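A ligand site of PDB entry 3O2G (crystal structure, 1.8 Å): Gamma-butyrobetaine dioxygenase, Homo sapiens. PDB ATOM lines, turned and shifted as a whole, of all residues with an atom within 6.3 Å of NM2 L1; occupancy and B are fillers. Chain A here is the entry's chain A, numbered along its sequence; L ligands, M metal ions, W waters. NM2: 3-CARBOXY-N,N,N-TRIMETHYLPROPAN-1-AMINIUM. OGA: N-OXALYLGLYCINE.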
ATOM      1  N   THR A 176       4.755  35.164  16.290  1.00  0.00           N
ATOM      2  CA  THR A 176       3.688  34.325  15.775  1.00  0.00           C
ATOM      3  C   THR A 176       2.572  34.112  16.836  1.00  0.00           C
ATOM      4  O   THR A 176       2.671  34.583  17.964  1.00  0.00           O
ATOM      5  CB  THR A 176       4.204  32.936  15.329  1.00  0.00           C
ATOM      6  OG1 THR A 176       4.534  32.121  16.474  1.00  0.00           O
ATOM      7  CG2 THR A 176       5.454  33.047  14.410  1.00  0.00           C
ATOM      8  N   TYR A 178       2.114  31.629  18.547  1.00  0.00           N
ATOM      9  CA  TYR A 178       2.636  30.884  19.724  1.00  0.00           C
ATOM     10  C   TYR A 178       3.465  31.781  20.630  1.00  0.00           C
ATOM     11  O   TYR A 178       3.918  31.354  21.699  1.00  0.00           O
ATOM     12  CB  TYR A 178       3.402  29.649  19.278  1.00  0.00           C
ATOM     13  CG  TYR A 178       2.485  28.599  18.755  1.00  0.00           C
ATOM     14  CD1 TYR A 178       1.736  27.829  19.623  1.00  0.00           C
ATOM     15  CD2 TYR A 178       2.288  28.431  17.375  1.00  0.00           C
ATOM     16  CE1 TYR A 178       0.848  26.876  19.133  1.00  0.00           C
ATOM     17  CE2 TYR A 178       1.367  27.495  16.885  1.00  0.00           C
ATOM     18  CZ  TYR A 178       0.669  26.703  17.784  1.00  0.00           C
ATOM     19  OH  TYR A 178      -0.214  25.760  17.338  1.00  0.00           O
ATOM     20  N   TRP A 182       8.334  30.728  22.929  1.00  0.00           N
ATOM     21  CA  TRP A 182       7.408  29.686  23.338  1.00  0.00           C
ATOM     22  C   TRP A 182       8.150  28.566  24.090  1.00  0.00           C
ATOM     23  O   TRP A 182       9.374  28.348  23.878  1.00  0.00           O
ATOM     24  CB  TRP A 182       6.630  29.137  22.148  1.00  0.00           C
ATOM     25  CG  TRP A 182       7.374  29.200  20.848  1.00  0.00           C
ATOM     26  CD1 TRP A 182       7.311  30.219  19.955  1.00  0.00           C
ATOM     27  CD2 TRP A 182       8.286  28.227  20.289  1.00  0.00           C
ATOM     28  NE1 TRP A 182       8.130  29.949  18.873  1.00  0.00           N
ATOM     29  CE2 TRP A 182       8.729  28.748  19.035  1.00  0.00           C
ATOM     30  CE3 TRP A 182       8.758  26.981  20.694  1.00  0.00           C
ATOM     31  CZ2 TRP A 182       9.620  28.067  18.219  1.00  0.00           C
ATOM     32  CZ3 TRP A 182       9.649  26.300  19.877  1.00  0.00           C
ATOM     33  CH2 TRP A 182      10.082  26.849  18.641  1.00  0.00           C
ATOM     34  N   VAL A 184       8.518  24.684  24.996  1.00  0.00           N
ATOM     35  CA  VAL A 184       8.268  23.333  24.559  1.00  0.00           C
ATOM     36  C   VAL A 184       8.341  22.449  25.795  1.00  0.00           C
ATOM     37  O   VAL A 184       9.421  22.168  26.286  1.00  0.00           O
ATOM     38  CB  VAL A 184       9.254  22.870  23.476  1.00  0.00           C
ATOM     39  CG1 VAL A 184       8.880  21.444  23.020  1.00  0.00           C
ATOM     40  CG2 VAL A 184       9.293  23.881  22.307  1.00  0.00           C
ATOM     41  N   ASN A 191      -2.270  22.592  22.914  1.00  0.00           N
ATOM     42  CA  ASN A 191      -2.770  23.172  21.684  1.00  0.00           C
ATOM     43  C   ASN A 191      -1.926  22.811  20.464  1.00  0.00           C
ATOM     44  O   ASN A 191      -2.165  23.282  19.335  1.00  0.00           O
ATOM     45  CB  ASN A 191      -2.925  24.702  21.810  1.00  0.00           C
ATOM     46  CG  ASN A 191      -1.596  25.423  21.965  1.00  0.00           C
ATOM     47  OD1 ASN A 191      -0.514  24.853  21.715  1.00  0.00           O
ATOM     48  ND2 ASN A 191      -1.665  26.723  22.310  1.00  0.00           N
ATOM     49  N   ASN A 192      -0.924  21.946  20.674  1.00  0.00           N
ATOM     50  CA  ASN A 192       0.014  21.604  19.607  1.00  0.00           C
ATOM     51  C   ASN A 192       0.732  20.296  20.003  1.00  0.00           C
ATOM     52  O   ASN A 192       1.014  20.097  21.177  1.00  0.00           O
ATOM     53  CB  ASN A 192       1.025  22.760  19.395  1.00  0.00           C
ATOM     54  CG  ASN A 192       1.841  22.624  18.094  1.00  0.00           C
ATOM     55  OD1 ASN A 192       2.743  21.800  18.015  1.00  0.00           O
ATOM     56  ND2 ASN A 192       1.546  23.471  17.080  1.00  0.00           N
ATOM     57  N   ALA A 194       3.671  19.444  19.648  1.00  0.00           N
ATOM     58  CA  ALA A 194       4.939  19.859  20.256  1.00  0.00           C
ATOM     59  C   ALA A 194       4.881  19.870  21.802  1.00  0.00           C
ATOM     60  O   ALA A 194       5.859  19.536  22.483  1.00  0.00           O
ATOM     61  CB  ALA A 194       5.326  21.263  19.749  1.00  0.00           C
ATOM     62  N   TYR A 195       3.731  20.266  22.356  1.00  0.00           N
ATOM     63  CA  TYR A 195       3.571  20.470  23.780  1.00  0.00           C
ATOM     64  C   TYR A 195       3.031  19.205  24.456  1.00  0.00           C
ATOM     65  O   TYR A 195       2.195  19.278  25.330  1.00  0.00           O
ATOM     66  CB  TYR A 195       2.670  21.659  24.050  1.00  0.00           C
ATOM     67  CG  TYR A 195       3.157  22.975  23.433  1.00  0.00           C
ATOM     68  CD1 TYR A 195       4.524  23.239  23.224  1.00  0.00           C
ATOM     69  CD2 TYR A 195       2.256  23.962  23.061  1.00  0.00           C
ATOM     70  CE1 TYR A 195       4.959  24.435  22.656  1.00  0.00           C
ATOM     71  CE2 TYR A 195       2.687  25.157  22.469  1.00  0.00           C
ATOM     72  CZ  TYR A 195       4.039  25.388  22.316  1.00  0.00           C
ATOM     73  OH  TYR A 195       4.533  26.562  21.774  1.00  0.00           O
ATOM     74  N   HIS A 203       9.947  17.352  10.529  1.00  0.00           N
ATOM     75  CA  HIS A 203       9.056  18.414  10.121  1.00  0.00           C
ATOM     76  C   HIS A 203       9.836  19.713   9.970  1.00  0.00           C
ATOM     77  O   HIS A 203      10.930  19.850  10.493  1.00  0.00           O
ATOM     78  CB  HIS A 203       7.917  18.659  11.125  1.00  0.00           C
ATOM     79  CG  HIS A 203       8.362  19.125  12.477  1.00  0.00           C
ATOM     80  ND1 HIS A 203       8.954  18.291  13.379  1.00  0.00           N
ATOM     81  CD2 HIS A 203       8.321  20.356  13.054  1.00  0.00           C
ATOM     82  CE1 HIS A 203       9.248  18.973  14.483  1.00  0.00           C
ATOM     83  NE2 HIS A 203       8.873  20.231  14.312  1.00  0.00           N
ATOM     84  N   THR A 204       9.237  20.652   9.252  1.00  0.00           N
ATOM     85  CA  THR A 204       9.545  22.082   9.326  1.00  0.00           C
ATOM     86  C   THR A 204       8.472  22.710  10.240  1.00  0.00           C
ATOM     87  O   THR A 204       7.372  22.217  10.308  1.00  0.00           O
ATOM     88  CB  THR A 204       9.558  22.752   7.902  1.00  0.00           C
ATOM     89  OG1 THR A 204       8.266  22.666   7.296  1.00  0.00           O
ATOM     90  CG2 THR A 204      10.583  22.075   6.994  1.00  0.00           C
ATOM     91  N   ASP A 205       8.817  23.782  10.957  1.00  0.00           N
ATOM     92  CA  ASP A 205       7.895  24.480  11.798  1.00  0.00           C
ATOM     93  C   ASP A 205       7.060  25.414  10.962  1.00  0.00           C
ATOM     94  O   ASP A 205       7.541  26.153  10.104  1.00  0.00           O
ATOM     95  CB  ASP A 205       8.628  25.278  12.891  1.00  0.00           C
ATOM     96  CG  ASP A 205       8.811  24.493  14.156  1.00  0.00           C
ATOM     97  OD1 ASP A 205       8.949  23.288  14.043  1.00  0.00           O
ATOM     98  OD2 ASP A 205       8.752  25.111  15.252  1.00  0.00           O
ATOM     99  N   TYR A 206       5.764  25.379  11.232  1.00  0.00           N
ATOM    100  CA  TYR A 206       4.821  26.399  10.803  1.00  0.00           C
ATOM    101  C   TYR A 206       4.519  26.474   9.288  1.00  0.00           C
ATOM    102  O   TYR A 206       4.335  27.553   8.746  1.00  0.00           O
ATOM    103  CB  TYR A 206       5.210  27.783  11.407  1.00  0.00           C
ATOM    104  CG  TYR A 206       4.163  28.427  12.322  1.00  0.00           C
ATOM    105  CD1 TYR A 206       4.564  29.177  13.436  1.00  0.00           C
ATOM    106  CD2 TYR A 206       2.788  28.308  12.068  1.00  0.00           C
ATOM    107  CE1 TYR A 206       3.674  29.781  14.229  1.00  0.00           C
ATOM    108  CE2 TYR A 206       1.859  28.917  12.911  1.00  0.00           C
ATOM    109  CZ  TYR A 206       2.320  29.652  13.994  1.00  0.00           C
ATOM    110  OH  TYR A 206       1.430  30.312  14.835  1.00  0.00           O
ATOM    111  N   PRO A 207       4.356  25.329   8.611  1.00  0.00           N
ATOM    112  CA  PRO A 207       3.852  25.403   7.245  1.00  0.00           C
ATOM    113  C   PRO A 207       2.388  25.899   7.207  1.00  0.00           C
ATOM    114  O   PRO A 207       1.895  26.263   6.160  1.00  0.00           O
ATOM    115  CB  PRO A 207       3.978  23.955   6.747  1.00  0.00           C
ATOM    116  CG  PRO A 207       3.886  23.147   7.969  1.00  0.00           C
ATOM    117  CD  PRO A 207       4.614  23.935   9.017  1.00  0.00           C
ATOM    118  N   ALA A 208       1.701  25.984   8.345  1.00  0.00           N
ATOM    119  CA  ALA A 208       0.373  26.600   8.374  1.00  0.00           C
ATOM    120  C   ALA A 208       0.414  28.091   8.020  1.00  0.00           C
ATOM    121  O   ALA A 208      -0.606  28.710   7.763  1.00  0.00           O
ATOM    122  CB  ALA A 208      -0.354  26.354   9.753  1.00  0.00           C
ATOM    123  N   GLN A 216      14.996  29.185  13.057  1.00  0.00           N
ATOM    124  CA  GLN A 216      14.484  28.743  14.338  1.00  0.00           C
ATOM    125  C   GLN A 216      15.621  28.732  15.381  1.00  0.00           C
ATOM    126  O   GLN A 216      16.742  28.328  15.091  1.00  0.00           O
ATOM    127  CB  GLN A 216      13.865  27.355  14.208  1.00  0.00           C
ATOM    128  CG  GLN A 216      13.222  26.891  15.469  1.00  0.00           C
ATOM    129  CD  GLN A 216      12.600  25.518  15.372  1.00  0.00           C
ATOM    130  OE1 GLN A 216      12.506  24.844  16.374  1.00  0.00           O
ATOM    131  NE2 GLN A 216      12.120  25.123  14.163  1.00  0.00           N
ATOM    132  N   ASP A 262      -4.096  25.263  11.450  1.00  0.00           N
ATOM    133  CA  ASP A 262      -3.812  25.341  12.891  1.00  0.00           C
ATOM    134  C   ASP A 262      -4.920  26.175  13.539  1.00  0.00           C
ATOM    135  O   ASP A 262      -5.092  27.353  13.212  1.00  0.00           O
ATOM    136  CB  ASP A 262      -2.443  25.962  13.129  1.00  0.00           C
ATOM    137  CG  ASP A 262      -1.891  25.692  14.508  1.00  0.00           C
ATOM    138  OD1 ASP A 262      -2.340  24.761  15.201  1.00  0.00           O
ATOM    139  OD2 ASP A 262      -0.966  26.432  14.882  1.00  0.00           O
ATOM    140  N   ASN A 293       4.866  19.596   7.896  1.00  0.00           N
ATOM    141  CA  ASN A 293       4.686  19.158   9.259  1.00  0.00           C
ATOM    142  C   ASN A 293       3.473  18.206   9.237  1.00  0.00           C
ATOM    143  O   ASN A 293       2.369  18.640   8.875  1.00  0.00           O
ATOM    144  CB  ASN A 293       4.415  20.329  10.183  1.00  0.00           C
ATOM    145  CG  ASN A 293       4.252  19.916  11.667  1.00  0.00           C
ATOM    146  OD1 ASN A 293       4.109  18.729  11.996  1.00  0.00           O
ATOM    147  ND2 ASN A 293       4.294  20.892  12.559  1.00  0.00           N
ATOM    148  N   THR A 296       0.245  19.164  11.264  1.00  0.00           N
ATOM    149  CA  THR A 296      -0.592  20.320  10.873  1.00  0.00           C
ATOM    150  C   THR A 296      -1.087  20.229   9.434  1.00  0.00           C
ATOM    151  O   THR A 296      -1.889  21.062   8.978  1.00  0.00           O
ATOM    152  CB  THR A 296       0.103  21.669  11.134  1.00  0.00           C
ATOM    153  OG1 THR A 296       1.232  21.783  10.267  1.00  0.00           O
ATOM    154  CG2 THR A 296       0.513  21.813  12.599  1.00  0.00           C
ATOM    155  N   TYR A 367      11.579  32.352  16.628  1.00  0.00           N
ATOM    156  CA  TYR A 367      11.819  32.423  15.193  1.00  0.00           C
ATOM    157  C   TYR A 367      12.393  33.773  14.791  1.00  0.00           C
ATOM    158  O   TYR A 367      12.231  34.776  15.498  1.00  0.00           O
ATOM    159  CB  TYR A 367      10.494  32.219  14.437  1.00  0.00           C
ATOM    160  CG  TYR A 367       9.746  30.907  14.721  1.00  0.00           C
ATOM    161  CD1 TYR A 367      10.290  29.663  14.413  1.00  0.00           C
ATOM    162  CD2 TYR A 367       8.446  30.933  15.225  1.00  0.00           C
ATOM    163  CE1 TYR A 367       9.589  28.476  14.636  1.00  0.00           C
ATOM    164  CE2 TYR A 367       7.718  29.770  15.438  1.00  0.00           C
ATOM    165  CZ  TYR A 367       8.299  28.523  15.134  1.00  0.00           C
ATOM    166  OH  TYR A 367       7.609  27.335  15.376  1.00  0.00           O
HETATM  167  N1  NM2 L   1       5.493  25.534  17.975  1.00  0.00           N
HETATM  168  C8  NM2 L   1       5.726  27.007  18.074  1.00  0.00           C
HETATM  169  O4  NM2 L   1       3.161  23.855  14.608  1.00  0.00           O
HETATM  170  C5  NM2 L   1       4.085  23.870  13.747  1.00  0.00           C
HETATM  171  O7  NM2 L   1       4.066  23.735  12.521  1.00  0.00           O
HETATM  172  C6  NM2 L   1       5.209  23.521  14.710  1.00  0.00           C
HETATM  173  C2  NM2 L   1       5.373  25.218  16.534  1.00  0.00           C
HETATM  174  C9  NM2 L   1       4.269  25.050  18.651  1.00  0.00           C
HETATM  175  C10 NM2 L   1       6.636  24.829  18.584  1.00  0.00           C
HETATM  176  C3  NM2 L   1       5.318  23.795  16.062  1.00  0.00           C
HETATM  177  C1  OGA L   2       8.625  21.672  18.015  1.00  0.00           C
HETATM  178  C2  OGA L   2       9.912  20.885  18.044  1.00  0.00           C
HETATM  179  C4  OGA L   2      11.690  19.772  19.205  1.00  0.00           C
HETATM  180  C5  OGA L   2      11.946  19.169  20.598  1.00  0.00           C
HETATM  181  O1  OGA L   2       8.187  22.053  19.126  1.00  0.00           O
HETATM  182  O2  OGA L   2       8.100  21.901  16.880  1.00  0.00           O
HETATM  183  O2' OGA L   2      10.408  20.549  16.962  1.00  0.00           O
HETATM  184  O3  OGA L   2      10.990  19.209  21.396  1.00  0.00           O
HETATM  185  N1  OGA L   2      10.437  20.540  19.218  1.00  0.00           N
HETATM  186  O4  OGA L   2      13.097  18.739  20.806  1.00  0.00           O
HETATM  187 ZN    ZN M   1       9.637  21.817  15.442  1.00  0.00          ZN
HETATM  188  O   HOH W   1       1.057  25.339  13.214  1.00  0.00           O
HETATM  189  O   HOH W   2       3.265  20.685  15.445  1.00  0.00           O
HETATM  190  O   HOH W   3       2.055  24.465  10.922  1.00  0.00           O
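ND2 of Asn 192 lies within hydrogen-bond range of O4 of NM2 L1, at 3.0 Å. ND2 of Asn 293 lies within hydrogen-bond range of O7 of NM2 L1 (2.9 Å). An oxygen (O7) of NM2 L1 sits at hydrogen-bond distance from the backbone NH of Tyr 206.
OH of Tyr 178 lies within hydrogen-bond range of OD2 of Asp 262 (2.7 Å). The side-chain hydroxyl (OH) of Tyr 178 is in hydrogen-bond range of the side-chain amide nitrogen (ND2) of Asn 192, at 2.9 Å. The backbone NH (N) of Tyr 178 lies close to the side-chain hydroxyl (OG1) of Thr 176. The side-chain carboxylate of Asp 205 lies within hydrogen-bond range of the side-chain hydroxyl of Tyr 367. The side-chain amide oxygen of Asn 192 is in hydrogen-bond range of the backbone NH of Ala 194 (3.0 Å).
Merely in contact with NM2 L1: Tyr 178 (3.7 Å), Trp 182 (3.6 Å), Ala 194 (3.97 Å), Tyr 195 (3.5 Å), Asp 205 (3.6 Å), Pro 207 (3.6 Å), Thr 296 (3.9 Å) and Tyr 367 (3.3 Å). Hydrophobic or aromatic side chains that line NM2 L1: Tyr 178, Trp 182, Ala 194, Tyr 195 and Pro 207. 11 residues have an atom within 4 Å of NM2 L1: Tyr 178, Trp 182, Asn 192, Ala 194, Tyr 195, Asp 205, Tyr 206, Pro 207, Asn 293, Thr 296 and Tyr 367.
Water W3 lies within hydrogen-bond range of O7 of NM2 L1, OG1 of Thr 296 and N of Ala 208. Water W1 lies within hydrogen-bond range of the side-chain carboxylate of Asp 262 (2.8 Å) and an oxygen (O4) of NM2 L1 (2.9 Å). Water W2 lies within hydrogen-bond range of OD1 of Asn 192, ND2 of Asn 293 and O4 of NM2 L1.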
